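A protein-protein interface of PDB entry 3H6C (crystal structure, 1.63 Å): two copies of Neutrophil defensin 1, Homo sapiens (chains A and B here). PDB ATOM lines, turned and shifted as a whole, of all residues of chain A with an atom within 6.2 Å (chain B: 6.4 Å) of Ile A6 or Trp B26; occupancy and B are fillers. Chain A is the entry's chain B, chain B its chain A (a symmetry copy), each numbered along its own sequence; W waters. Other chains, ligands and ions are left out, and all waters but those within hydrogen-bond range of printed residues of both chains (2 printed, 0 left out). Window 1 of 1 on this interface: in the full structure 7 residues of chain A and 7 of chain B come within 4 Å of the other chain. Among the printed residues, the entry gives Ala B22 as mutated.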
ATOM      1  N   CYS A   4      -1.674 -11.849 -33.134  1.00  0.00           N
ATOM      2  CA  CYS A   4      -1.543 -12.505 -31.841  1.00  0.00           C
ATOM      3  C   CYS A   4      -0.882 -13.874 -32.080  1.00  0.00           C
ATOM      4  O   CYS A   4      -1.351 -14.658 -32.913  1.00  0.00           O
ATOM      5  CB  CYS A   4      -2.928 -12.637 -31.172  1.00  0.00           C
ATOM      6  SG  CYS A   4      -3.560 -10.996 -30.743  1.00  0.00           S
ATOM      7  N   ARG A   5       0.224 -14.152 -31.375  1.00  0.00           N
ATOM      8  CA  ARG A   5       0.962 -15.405 -31.606  1.00  0.00           C
ATOM      9  C   ARG A   5       1.354 -16.052 -30.300  1.00  0.00           C
ATOM     10  O   ARG A   5       1.687 -15.353 -29.336  1.00  0.00           O
ATOM     11  CB  ARG A   5       2.246 -15.155 -32.420  1.00  0.00           C
ATOM     12  CG  ARG A   5       1.982 -14.547 -33.781  1.00  0.00           C
ATOM     13  CD  ARG A   5       3.230 -14.639 -34.659  1.00  0.00           C
ATOM     14  NE  ARG A   5       3.122 -13.795 -35.846  1.00  0.00           N
ATOM     15  CZ  ARG A   5       2.443 -14.142 -36.935  1.00  0.00           C
ATOM     16  NH1 ARG A   5       1.804 -15.304 -36.983  1.00  0.00           N
ATOM     17  NH2 ARG A   5       2.402 -13.327 -37.988  1.00  0.00           N
ATOM     18  N   ILE A   6       1.341 -17.392 -30.285  1.00  0.00           N
ATOM     19  CA  ILE A   6       1.874 -18.208 -29.163  1.00  0.00           C
ATOM     20  C   ILE A   6       3.028 -19.115 -29.638  1.00  0.00           C
ATOM     21  O   ILE A   6       2.870 -19.842 -30.623  1.00  0.00           O
ATOM     22  CB  ILE A   6       0.730 -19.034 -28.462  1.00  0.00           C
ATOM     23  CG1 ILE A   6      -0.280 -18.090 -27.766  1.00  0.00           C
ATOM     24  CG2 ILE A   6       1.306 -20.119 -27.492  1.00  0.00           C
ATOM     25  CD1 ILE A   6      -1.567 -18.843 -27.320  1.00  0.00           C
ATOM     26  N   PRO A   7       4.174 -19.134 -28.900  1.00  0.00           N
ATOM     27  CA  PRO A   7       4.452 -18.400 -27.655  1.00  0.00           C
ATOM     28  C   PRO A   7       5.155 -17.085 -27.931  1.00  0.00           C
ATOM     29  O   PRO A   7       5.340 -16.283 -27.005  1.00  0.00           O
ATOM     30  CB  PRO A   7       5.422 -19.342 -26.922  1.00  0.00           C
ATOM     31  CG  PRO A   7       6.144 -19.978 -28.012  1.00  0.00           C
ATOM     32  CD  PRO A   7       5.121 -20.262 -29.065  1.00  0.00           C
ATOM     33  N   ALA A   8       5.554 -16.855 -29.179  1.00  0.00           N
ATOM     34  CA  ALA A   8       6.343 -15.655 -29.502  1.00  0.00           C
ATOM     35  C   ALA A   8       6.061 -15.115 -30.873  1.00  0.00           C
ATOM     36  O   ALA A   8       5.525 -15.816 -31.731  1.00  0.00           O
ATOM     37  CB  ALA A   8       7.805 -15.966 -29.410  1.00  0.00           C
ATOM     38  N   ARG A  24      -6.749 -17.421 -23.630  1.00  0.00           N
ATOM     39  CA  ARG A  24      -5.294 -17.572 -23.617  1.00  0.00           C
ATOM     40  C   ARG A  24      -4.602 -16.227 -23.762  1.00  0.00           C
ATOM     41  O   ARG A  24      -5.208 -15.228 -24.180  1.00  0.00           O
ATOM     42  CB  ARG A  24      -4.807 -18.504 -24.747  1.00  0.00           C
ATOM     43  CG  ARG A  24      -5.041 -20.017 -24.525  1.00  0.00           C
ATOM     44  CD  ARG A  24      -6.483 -20.405 -24.741  1.00  0.00           C
ATOM     45  NE  ARG A  24      -6.581 -21.844 -24.983  1.00  0.00           N
ATOM     46  CZ  ARG A  24      -7.715 -22.435 -25.326  1.00  0.00           C
ATOM     47  NH1 ARG A  24      -8.806 -21.690 -25.514  1.00  0.00           N
ATOM     48  NH2 ARG A  24      -7.744 -23.746 -25.528  1.00  0.00           N
ATOM     49  N   LEU A  25      -3.352 -16.202 -23.349  1.00  0.00           N
ATOM     50  CA  LEU A  25      -2.476 -15.035 -23.498  1.00  0.00           C
ATOM     51  C   LEU A  25      -1.563 -15.269 -24.693  1.00  0.00           C
ATOM     52  O   LEU A  25      -1.047 -16.425 -24.859  1.00  0.00           O
ATOM     53  CB  LEU A  25      -1.622 -14.902 -22.252  1.00  0.00           C
ATOM     54  CG  LEU A  25      -2.448 -14.510 -21.042  1.00  0.00           C
ATOM     55  CD1 LEU A  25      -1.617 -14.705 -19.795  1.00  0.00           C
ATOM     56  CD2 LEU A  25      -2.850 -13.007 -21.155  1.00  0.00           C
ATOM     57  N   TRP A  26      -1.410 -14.233 -25.503  1.00  0.00           N
ATOM     58  CA  TRP A  26      -0.622 -14.275 -26.742  1.00  0.00           C
ATOM     59  C   TRP A  26       0.340 -13.100 -26.797  1.00  0.00           C
ATOM     60  O   TRP A  26       0.090 -12.085 -26.179  1.00  0.00           O
ATOM     61  CB  TRP A  26      -1.556 -14.140 -27.949  1.00  0.00           C
ATOM     62  CG  TRP A  26      -2.769 -15.076 -27.973  1.00  0.00           C
ATOM     63  CD1 TRP A  26      -3.870 -15.074 -27.115  1.00  0.00           C
ATOM     64  CD2 TRP A  26      -3.017 -16.135 -28.931  1.00  0.00           C
ATOM     65  NE1 TRP A  26      -4.768 -16.074 -27.492  1.00  0.00           N
ATOM     66  CE2 TRP A  26      -4.266 -16.742 -28.582  1.00  0.00           C
ATOM     67  CE3 TRP A  26      -2.304 -16.634 -30.037  1.00  0.00           C
ATOM     68  CZ2 TRP A  26      -4.802 -17.824 -29.305  1.00  0.00           C
ATOM     69  CZ3 TRP A  26      -2.847 -17.733 -30.744  1.00  0.00           C
ATOM     70  CH2 TRP A  26      -4.085 -18.302 -30.372  1.00  0.00           C
ATOM     71  N   ALA A  27       1.426 -13.265 -27.528  1.00  0.00           N
ATOM     72  CA  ALA A  27       2.280 -12.124 -27.862  1.00  0.00           C
ATOM     73  C   ALA A  27       1.560 -11.252 -28.868  1.00  0.00           C
ATOM     74  O   ALA A  27       0.982 -11.771 -29.822  1.00  0.00           O
ATOM     75  CB  ALA A  27       3.561 -12.626 -28.455  1.00  0.00           C
ATOM     76  N   CYS B   4      -2.820 -27.299 -35.309  1.00  0.00           N
ATOM     77  CA  CYS B   4      -3.294 -26.992 -33.952  1.00  0.00           C
ATOM     78  C   CYS B   4      -3.816 -25.550 -33.957  1.00  0.00           C
ATOM     79  O   CYS B   4      -3.140 -24.645 -34.456  1.00  0.00           O
ATOM     80  CB  CYS B   4      -2.140 -27.137 -32.948  1.00  0.00           C
ATOM     81  SG  CYS B   4      -1.639 -28.855 -32.891  1.00  0.00           S
ATOM     82  N   ARG B   5      -5.000 -25.329 -33.401  1.00  0.00           N
ATOM     83  CA  ARG B   5      -5.652 -24.023 -33.486  1.00  0.00           C
ATOM     84  C   ARG B   5      -6.338 -23.712 -32.178  1.00  0.00           C
ATOM     85  O   ARG B   5      -6.863 -24.619 -31.509  1.00  0.00           O
ATOM     86  CB  ARG B   5      -6.710 -24.010 -34.606  1.00  0.00           C
ATOM     87  CG  ARG B   5      -6.168 -24.311 -36.016  1.00  0.00           C
ATOM     88  CD  ARG B   5      -7.226 -23.915 -37.023  1.00  0.00           C
ATOM     89  NE  ARG B   5      -7.004 -24.437 -38.378  1.00  0.00           N
ATOM     90  CZ  ARG B   5      -6.247 -23.832 -39.293  1.00  0.00           C
ATOM     91  NH1 ARG B   5      -5.595 -22.725 -38.980  1.00  0.00           N
ATOM     92  NH2 ARG B   5      -6.119 -24.357 -40.502  1.00  0.00           N
ATOM     93  N   ILE B   6      -6.373 -22.428 -31.835  1.00  0.00           N
ATOM     94  CA  ILE B   6      -7.171 -21.997 -30.692  1.00  0.00           C
ATOM     95  C   ILE B   6      -8.201 -20.948 -31.204  1.00  0.00           C
ATOM     96  O   ILE B   6      -7.834 -20.005 -31.935  1.00  0.00           O
ATOM     97  CB  ILE B   6      -6.261 -21.391 -29.596  1.00  0.00           C
ATOM     98  CG1 ILE B   6      -5.564 -22.483 -28.789  1.00  0.00           C
ATOM     99  CG2 ILE B   6      -7.056 -20.508 -28.616  1.00  0.00           C
ATOM    100  CD1 ILE B   6      -4.328 -21.940 -28.053  1.00  0.00           C
ATOM    101  N   PRO B   7      -9.480 -21.056 -30.778  1.00  0.00           N
ATOM    102  CA  PRO B   7     -10.011 -22.024 -29.806  1.00  0.00           C
ATOM    103  C   PRO B   7     -10.683 -23.192 -30.479  1.00  0.00           C
ATOM    104  O   PRO B   7     -11.154 -24.086 -29.792  1.00  0.00           O
ATOM    105  CB  PRO B   7     -11.093 -21.221 -29.052  1.00  0.00           C
ATOM    106  CG  PRO B   7     -11.598 -20.238 -30.055  1.00  0.00           C
ATOM    107  CD  PRO B   7     -10.297 -19.813 -30.828  1.00  0.00           C
ATOM    108  N   ARG B  15     -12.373 -31.373 -35.769  1.00  0.00           N
ATOM    109  CA  ARG B  15     -11.496 -31.556 -34.615  1.00  0.00           C
ATOM    110  C   ARG B  15     -11.344 -33.028 -34.307  1.00  0.00           C
ATOM    111  O   ARG B  15     -12.332 -33.704 -34.035  1.00  0.00           O
ATOM    112  CB  ARG B  15     -12.070 -30.859 -33.390  1.00  0.00           C
ATOM    113  CG  ARG B  15     -11.156 -30.966 -32.232  1.00  0.00           C
ATOM    114  CD  ARG B  15     -11.606 -30.095 -31.126  1.00  0.00           C
ATOM    115  NE  ARG B  15     -10.649 -30.184 -30.044  1.00  0.00           N
ATOM    116  CZ  ARG B  15     -10.684 -29.435 -28.937  1.00  0.00           C
ATOM    117  NH1 ARG B  15     -11.644 -28.527 -28.737  1.00  0.00           N
ATOM    118  NH2 ARG B  15      -9.753 -29.599 -28.019  1.00  0.00           N
ATOM    119  N   GLY B  17      -8.917 -34.098 -31.970  1.00  0.00           N
ATOM    120  CA  GLY B  17      -8.254 -34.277 -30.671  1.00  0.00           C
ATOM    121  C   GLY B  17      -7.779 -32.940 -30.163  1.00  0.00           C
ATOM    122  O   GLY B  17      -8.294 -31.874 -30.546  1.00  0.00           O
ATOM    123  N   THR B  18      -6.738 -33.012 -29.361  1.00  0.00           N
ATOM    124  CA  THR B  18      -6.168 -31.832 -28.715  1.00  0.00           C
ATOM    125  C   THR B  18      -4.647 -31.836 -28.828  1.00  0.00           C
ATOM    126  O   THR B  18      -4.001 -32.870 -28.898  1.00  0.00           O
ATOM    127  CB  THR B  18      -6.611 -31.818 -27.213  1.00  0.00           C
ATOM    128  OG1 THR B  18      -8.033 -31.777 -27.178  1.00  0.00           O
ATOM    129  CG2 THR B  18      -6.061 -30.647 -26.458  1.00  0.00           C
ATOM    130  N   CYS B  19      -4.066 -30.643 -28.892  1.00  0.00           N
ATOM    131  CA  CYS B  19      -2.608 -30.557 -28.894  1.00  0.00           C
ATOM    132  C   CYS B  19      -2.197 -29.875 -27.617  1.00  0.00           C
ATOM    133  O   CYS B  19      -2.885 -28.941 -27.121  1.00  0.00           O
ATOM    134  CB  CYS B  19      -2.103 -29.634 -30.002  1.00  0.00           C
ATOM    135  SG  CYS B  19      -2.939 -29.796 -31.604  1.00  0.00           S
ATOM    136  N   ILE B  20      -1.030 -30.255 -27.131  1.00  0.00           N
ATOM    137  CA  ILE B  20      -0.356 -29.541 -26.054  1.00  0.00           C
ATOM    138  C   ILE B  20       0.885 -28.958 -26.700  1.00  0.00           C
ATOM    139  O   ILE B  20       1.764 -29.678 -27.175  1.00  0.00           O
ATOM    140  CB  ILE B  20       0.032 -30.485 -24.891  1.00  0.00           C
ATOM    141  CG1 ILE B  20      -1.224 -30.999 -24.186  1.00  0.00           C
ATOM    142  CG2 ILE B  20       0.913 -29.740 -23.878  1.00  0.00           C
ATOM    143  CD1 ILE B  20      -1.070 -32.411 -23.802  1.00  0.00           C
ATOM    144  N   TYR B  21       0.946 -27.625 -26.713  1.00  0.00           N
ATOM    145  CA  TYR B  21       2.038 -26.923 -27.373  1.00  0.00           C
ATOM    146  C   TYR B  21       2.280 -25.583 -26.700  1.00  0.00           C
ATOM    147  O   TYR B  21       1.333 -24.808 -26.494  1.00  0.00           O
ATOM    148  CB  TYR B  21       1.731 -26.723 -28.881  1.00  0.00           C
ATOM    149  CG  TYR B  21       2.697 -25.742 -29.566  1.00  0.00           C
ATOM    150  CD1 TYR B  21       4.038 -26.055 -29.694  1.00  0.00           C
ATOM    151  CD2 TYR B  21       2.261 -24.491 -30.028  1.00  0.00           C
ATOM    152  CE1 TYR B  21       4.945 -25.137 -30.277  1.00  0.00           C
ATOM    153  CE2 TYR B  21       3.142 -23.582 -30.621  1.00  0.00           C
ATOM    154  CZ  TYR B  21       4.480 -23.920 -30.745  1.00  0.00           C
ATOM    155  OH  TYR B  21       5.361 -23.032 -31.350  1.00  0.00           O
ATOM    156  N   ALA B  22       3.526 -25.351 -26.294  1.00  0.00           N
ATOM    157  CA  ALA B  22       3.926 -24.083 -25.699  1.00  0.00           C
ATOM    158  C   ALA B  22       3.113 -23.728 -24.460  1.00  0.00           C
ATOM    159  O   ALA B  22       2.866 -22.531 -24.198  1.00  0.00           O
ATOM    160  CB  ALA B  22       3.853 -22.954 -26.740  1.00  0.00           C
ATOM    161  N   GLY B  23       2.722 -24.750 -23.691  1.00  0.00           N
ATOM    162  CA  GLY B  23       2.004 -24.583 -22.415  1.00  0.00           C
ATOM    163  C   GLY B  23       0.522 -24.232 -22.532  1.00  0.00           C
ATOM    164  O   GLY B  23      -0.107 -23.867 -21.528  1.00  0.00           O
ATOM    165  N   ARG B  24      -0.013 -24.308 -23.748  1.00  0.00           N
ATOM    166  CA  ARG B  24      -1.429 -24.139 -23.986  1.00  0.00           C
ATOM    167  C   ARG B  24      -2.029 -25.395 -24.644  1.00  0.00           C
ATOM    168  O   ARG B  24      -1.293 -26.246 -25.228  1.00  0.00           O
ATOM    169  CB  ARG B  24      -1.726 -22.959 -24.923  1.00  0.00           C
ATOM    170  CG  ARG B  24      -1.543 -21.562 -24.354  1.00  0.00           C
ATOM    171  CD  ARG B  24      -0.116 -21.208 -24.110  1.00  0.00           C
ATOM    172  NE  ARG B  24      -0.070 -19.769 -23.912  1.00  0.00           N
ATOM    173  CZ  ARG B  24       1.067 -19.080 -23.880  1.00  0.00           C
ATOM    174  NH1 ARG B  24       2.217 -19.718 -24.054  1.00  0.00           N
ATOM    175  NH2 ARG B  24       1.089 -17.759 -23.679  1.00  0.00           N
ATOM    176  N   LEU B  25      -3.369 -25.451 -24.611  1.00  0.00           N
ATOM    177  CA  LEU B  25      -4.198 -26.532 -25.152  1.00  0.00           C
ATOM    178  C   LEU B  25      -4.897 -26.046 -26.430  1.00  0.00           C
ATOM    179  O   LEU B  25      -5.567 -25.001 -26.416  1.00  0.00           O
ATOM    180  CB  LEU B  25      -5.265 -26.892 -24.118  1.00  0.00           C
ATOM    181  CG  LEU B  25      -5.965 -28.242 -24.232  1.00  0.00           C
ATOM    182  CD1 LEU B  25      -4.938 -29.375 -24.156  1.00  0.00           C
ATOM    183  CD2 LEU B  25      -6.929 -28.383 -23.091  1.00  0.00           C
ATOM    184  N   TRP B  26      -4.713 -26.789 -27.518  1.00  0.00           N
ATOM    185  CA  TRP B  26      -5.218 -26.405 -28.837  1.00  0.00           C
ATOM    186  C   TRP B  26      -6.135 -27.482 -29.368  1.00  0.00           C
ATOM    187  O   TRP B  26      -6.040 -28.646 -28.963  1.00  0.00           O
ATOM    188  CB  TRP B  26      -4.066 -26.280 -29.865  1.00  0.00           C
ATOM    189  CG  TRP B  26      -2.898 -25.406 -29.394  1.00  0.00           C
ATOM    190  CD1 TRP B  26      -2.030 -25.665 -28.358  1.00  0.00           C
ATOM    191  CD2 TRP B  26      -2.516 -24.139 -29.941  1.00  0.00           C
ATOM    192  NE1 TRP B  26      -1.133 -24.608 -28.235  1.00  0.00           N
ATOM    193  CE2 TRP B  26      -1.417 -23.676 -29.197  1.00  0.00           C
ATOM    194  CE3 TRP B  26      -3.004 -23.350 -30.987  1.00  0.00           C
ATOM    195  CZ2 TRP B  26      -0.802 -22.451 -29.461  1.00  0.00           C
ATOM    196  CZ3 TRP B  26      -2.385 -22.110 -31.254  1.00  0.00           C
ATOM    197  CH2 TRP B  26      -1.286 -21.690 -30.498  1.00  0.00           C
ATOM    198  N   ALA B  27      -7.014 -27.087 -30.270  1.00  0.00           N
ATOM    199  CA  ALA B  27      -7.738 -28.075 -31.054  1.00  0.00           C
ATOM    200  C   ALA B  27      -6.842 -28.664 -32.117  1.00  0.00           C
ATOM    201  O   ALA B  27      -6.128 -27.943 -32.783  1.00  0.00           O
ATOM    202  CB  ALA B  27      -8.948 -27.401 -31.678  1.00  0.00           C
ATOM    203  N   PHE B  28      -6.884 -29.999 -32.272  1.00  0.00           N
ATOM    204  CA  PHE B  28      -6.179 -30.671 -33.345  1.00  0.00           C
ATOM    205  C   PHE B  28      -7.171 -30.880 -34.484  1.00  0.00           C
ATOM    206  O   PHE B  28      -8.181 -31.550 -34.314  1.00  0.00           O
ATOM    207  CB  PHE B  28      -5.600 -31.986 -32.819  1.00  0.00           C
ATOM    208  CG  PHE B  28      -4.902 -32.807 -33.894  1.00  0.00           C
ATOM    209  CD1 PHE B  28      -3.808 -32.288 -34.580  1.00  0.00           C
ATOM    210  CD2 PHE B  28      -5.367 -34.072 -34.227  1.00  0.00           C
ATOM    211  CE1 PHE B  28      -3.187 -33.019 -35.608  1.00  0.00           C
ATOM    212  CE2 PHE B  28      -4.727 -34.825 -35.249  1.00  0.00           C
ATOM    213  CZ  PHE B  28      -3.650 -34.289 -35.926  1.00  0.00           C
HETATM  214  O   HOH W   1      -2.237 -18.656 -22.113  1.00  0.00           O
HETATM  215  O   HOH W   2      -4.709 -23.311 -23.095  1.00  0.00           O
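NH2 of Arg A24 sits at hydrogen-bond distance from O of Leu B25, at 2.7 Å.
The backbone carbonyl oxygen of Leu A25 lies within hydrogen-bond range of the guanidinium group of Arg B24.
The indole nitrogen (NE1) of Trp A26 lies close to the backbone carbonyl oxygen (O) of Arg A24, at 3.4 Å.
The backbone carbonyl oxygen (O) of Trp B26 sits at hydrogen-bond distance from the backbone NH (N) of Cys B19, 2.8 Å away.
The backbone carbonyl oxygen (O) of Tyr B21 sits at hydrogen-bond distance from the indole nitrogen (NE1) of Trp B26 (3.0 Å).
NH1 of Arg B24 sits at hydrogen-bond distance from O of Ala B22 (2.9 Å).
The backbone carbonyl oxygen (O) of Arg B24 lies close to the indole nitrogen (NE1) of Trp B26, 3.4 Å away.
SG of Cys B4 is disulfide-bonded to SG of Cys B19 (2.1 Å).
Ile A6 touches Tyr B21.
Ile A6 touches Ala B22 (CG2 to CB, 3.9 Å).
Ile A6 touches Arg B24 (CG2 to NH1, 3.6 Å).
Ile A6 touches Trp B26.
Tyr B21 touches Pro A7 (OH to CD, 3.6 Å).
Pro A7 touches Ala B22 (CD to CB, 3.8 Å).
Arg A24 touches Ile B6.
Arg B24 touches Arg A24.
Ile B6 touches Trp A26.
Ile A6 touches just these residues of chain B: Tyr B21 (3.7 Å), Ala B22 (3.9 Å), Arg B24 (3.6 Å) and Trp B26 (3.7 Å).
Trp B26 touches just one residue of chain A: Ile A6.
Printed residues of chain B within 4 Å of Arg A24: Ile B6 (3.8 Å), Arg B24 (3.8 Å) and Leu B25 (2.7 Å).
Of the printed residues of chain B, Leu A25 touches Arg B24 (2.8 Å).
Printed residues of chain A within 4 Å of Ala B22: Ile A6 and Pro A7.
Gly B17 touches none of the printed residues of chain A.
Ala A27 touches none of the printed residues of chain B.
The nearest printed residue of chain A that does not touch Arg B24 is Pro A7 (4.3 Å).
Of the 9 printed residues of chain A, 5 touch a printed residue of chain B.
Hydrophobic or aromatic side chains of chain B within 4 Å of the printed part of chain A: Ile B6, Tyr B21, Ala B22 and Trp B26.
Along chain B the printed residues that touch a printed residue of chain A span positions 6 to 26.
Among the printed residues, 11 pairs touch across the chains.
Ile A6 touches Arg B24, and with the chains exchanged Arg A24 touches Ile B6.
Ile A6 touches Trp B26, and with the chains exchanged Trp A26 touches Ile B6.
Arg B24 touches its own counterpart, Arg A24.
Arg A24 touches Leu B25, and with the chains exchanged Leu A25 touches Arg B24.
Positions printed for both chains: 4, 5, 6, 7, 24, 25, 26 and 27.
Of the 11 pairs that touch across the chains among the printed residues, 7 have their exchanged pair printed and touching as well.
Water W2 lies within hydrogen-bond range of the backbone NH (N) of Leu B25 (2.9 Å) and the guanidinium group (NE) of Arg A24 (3.0 Å).
Water W1 bridges N of Leu A25 (3.0 Å) and NE of Arg B24 (3.0 Å).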
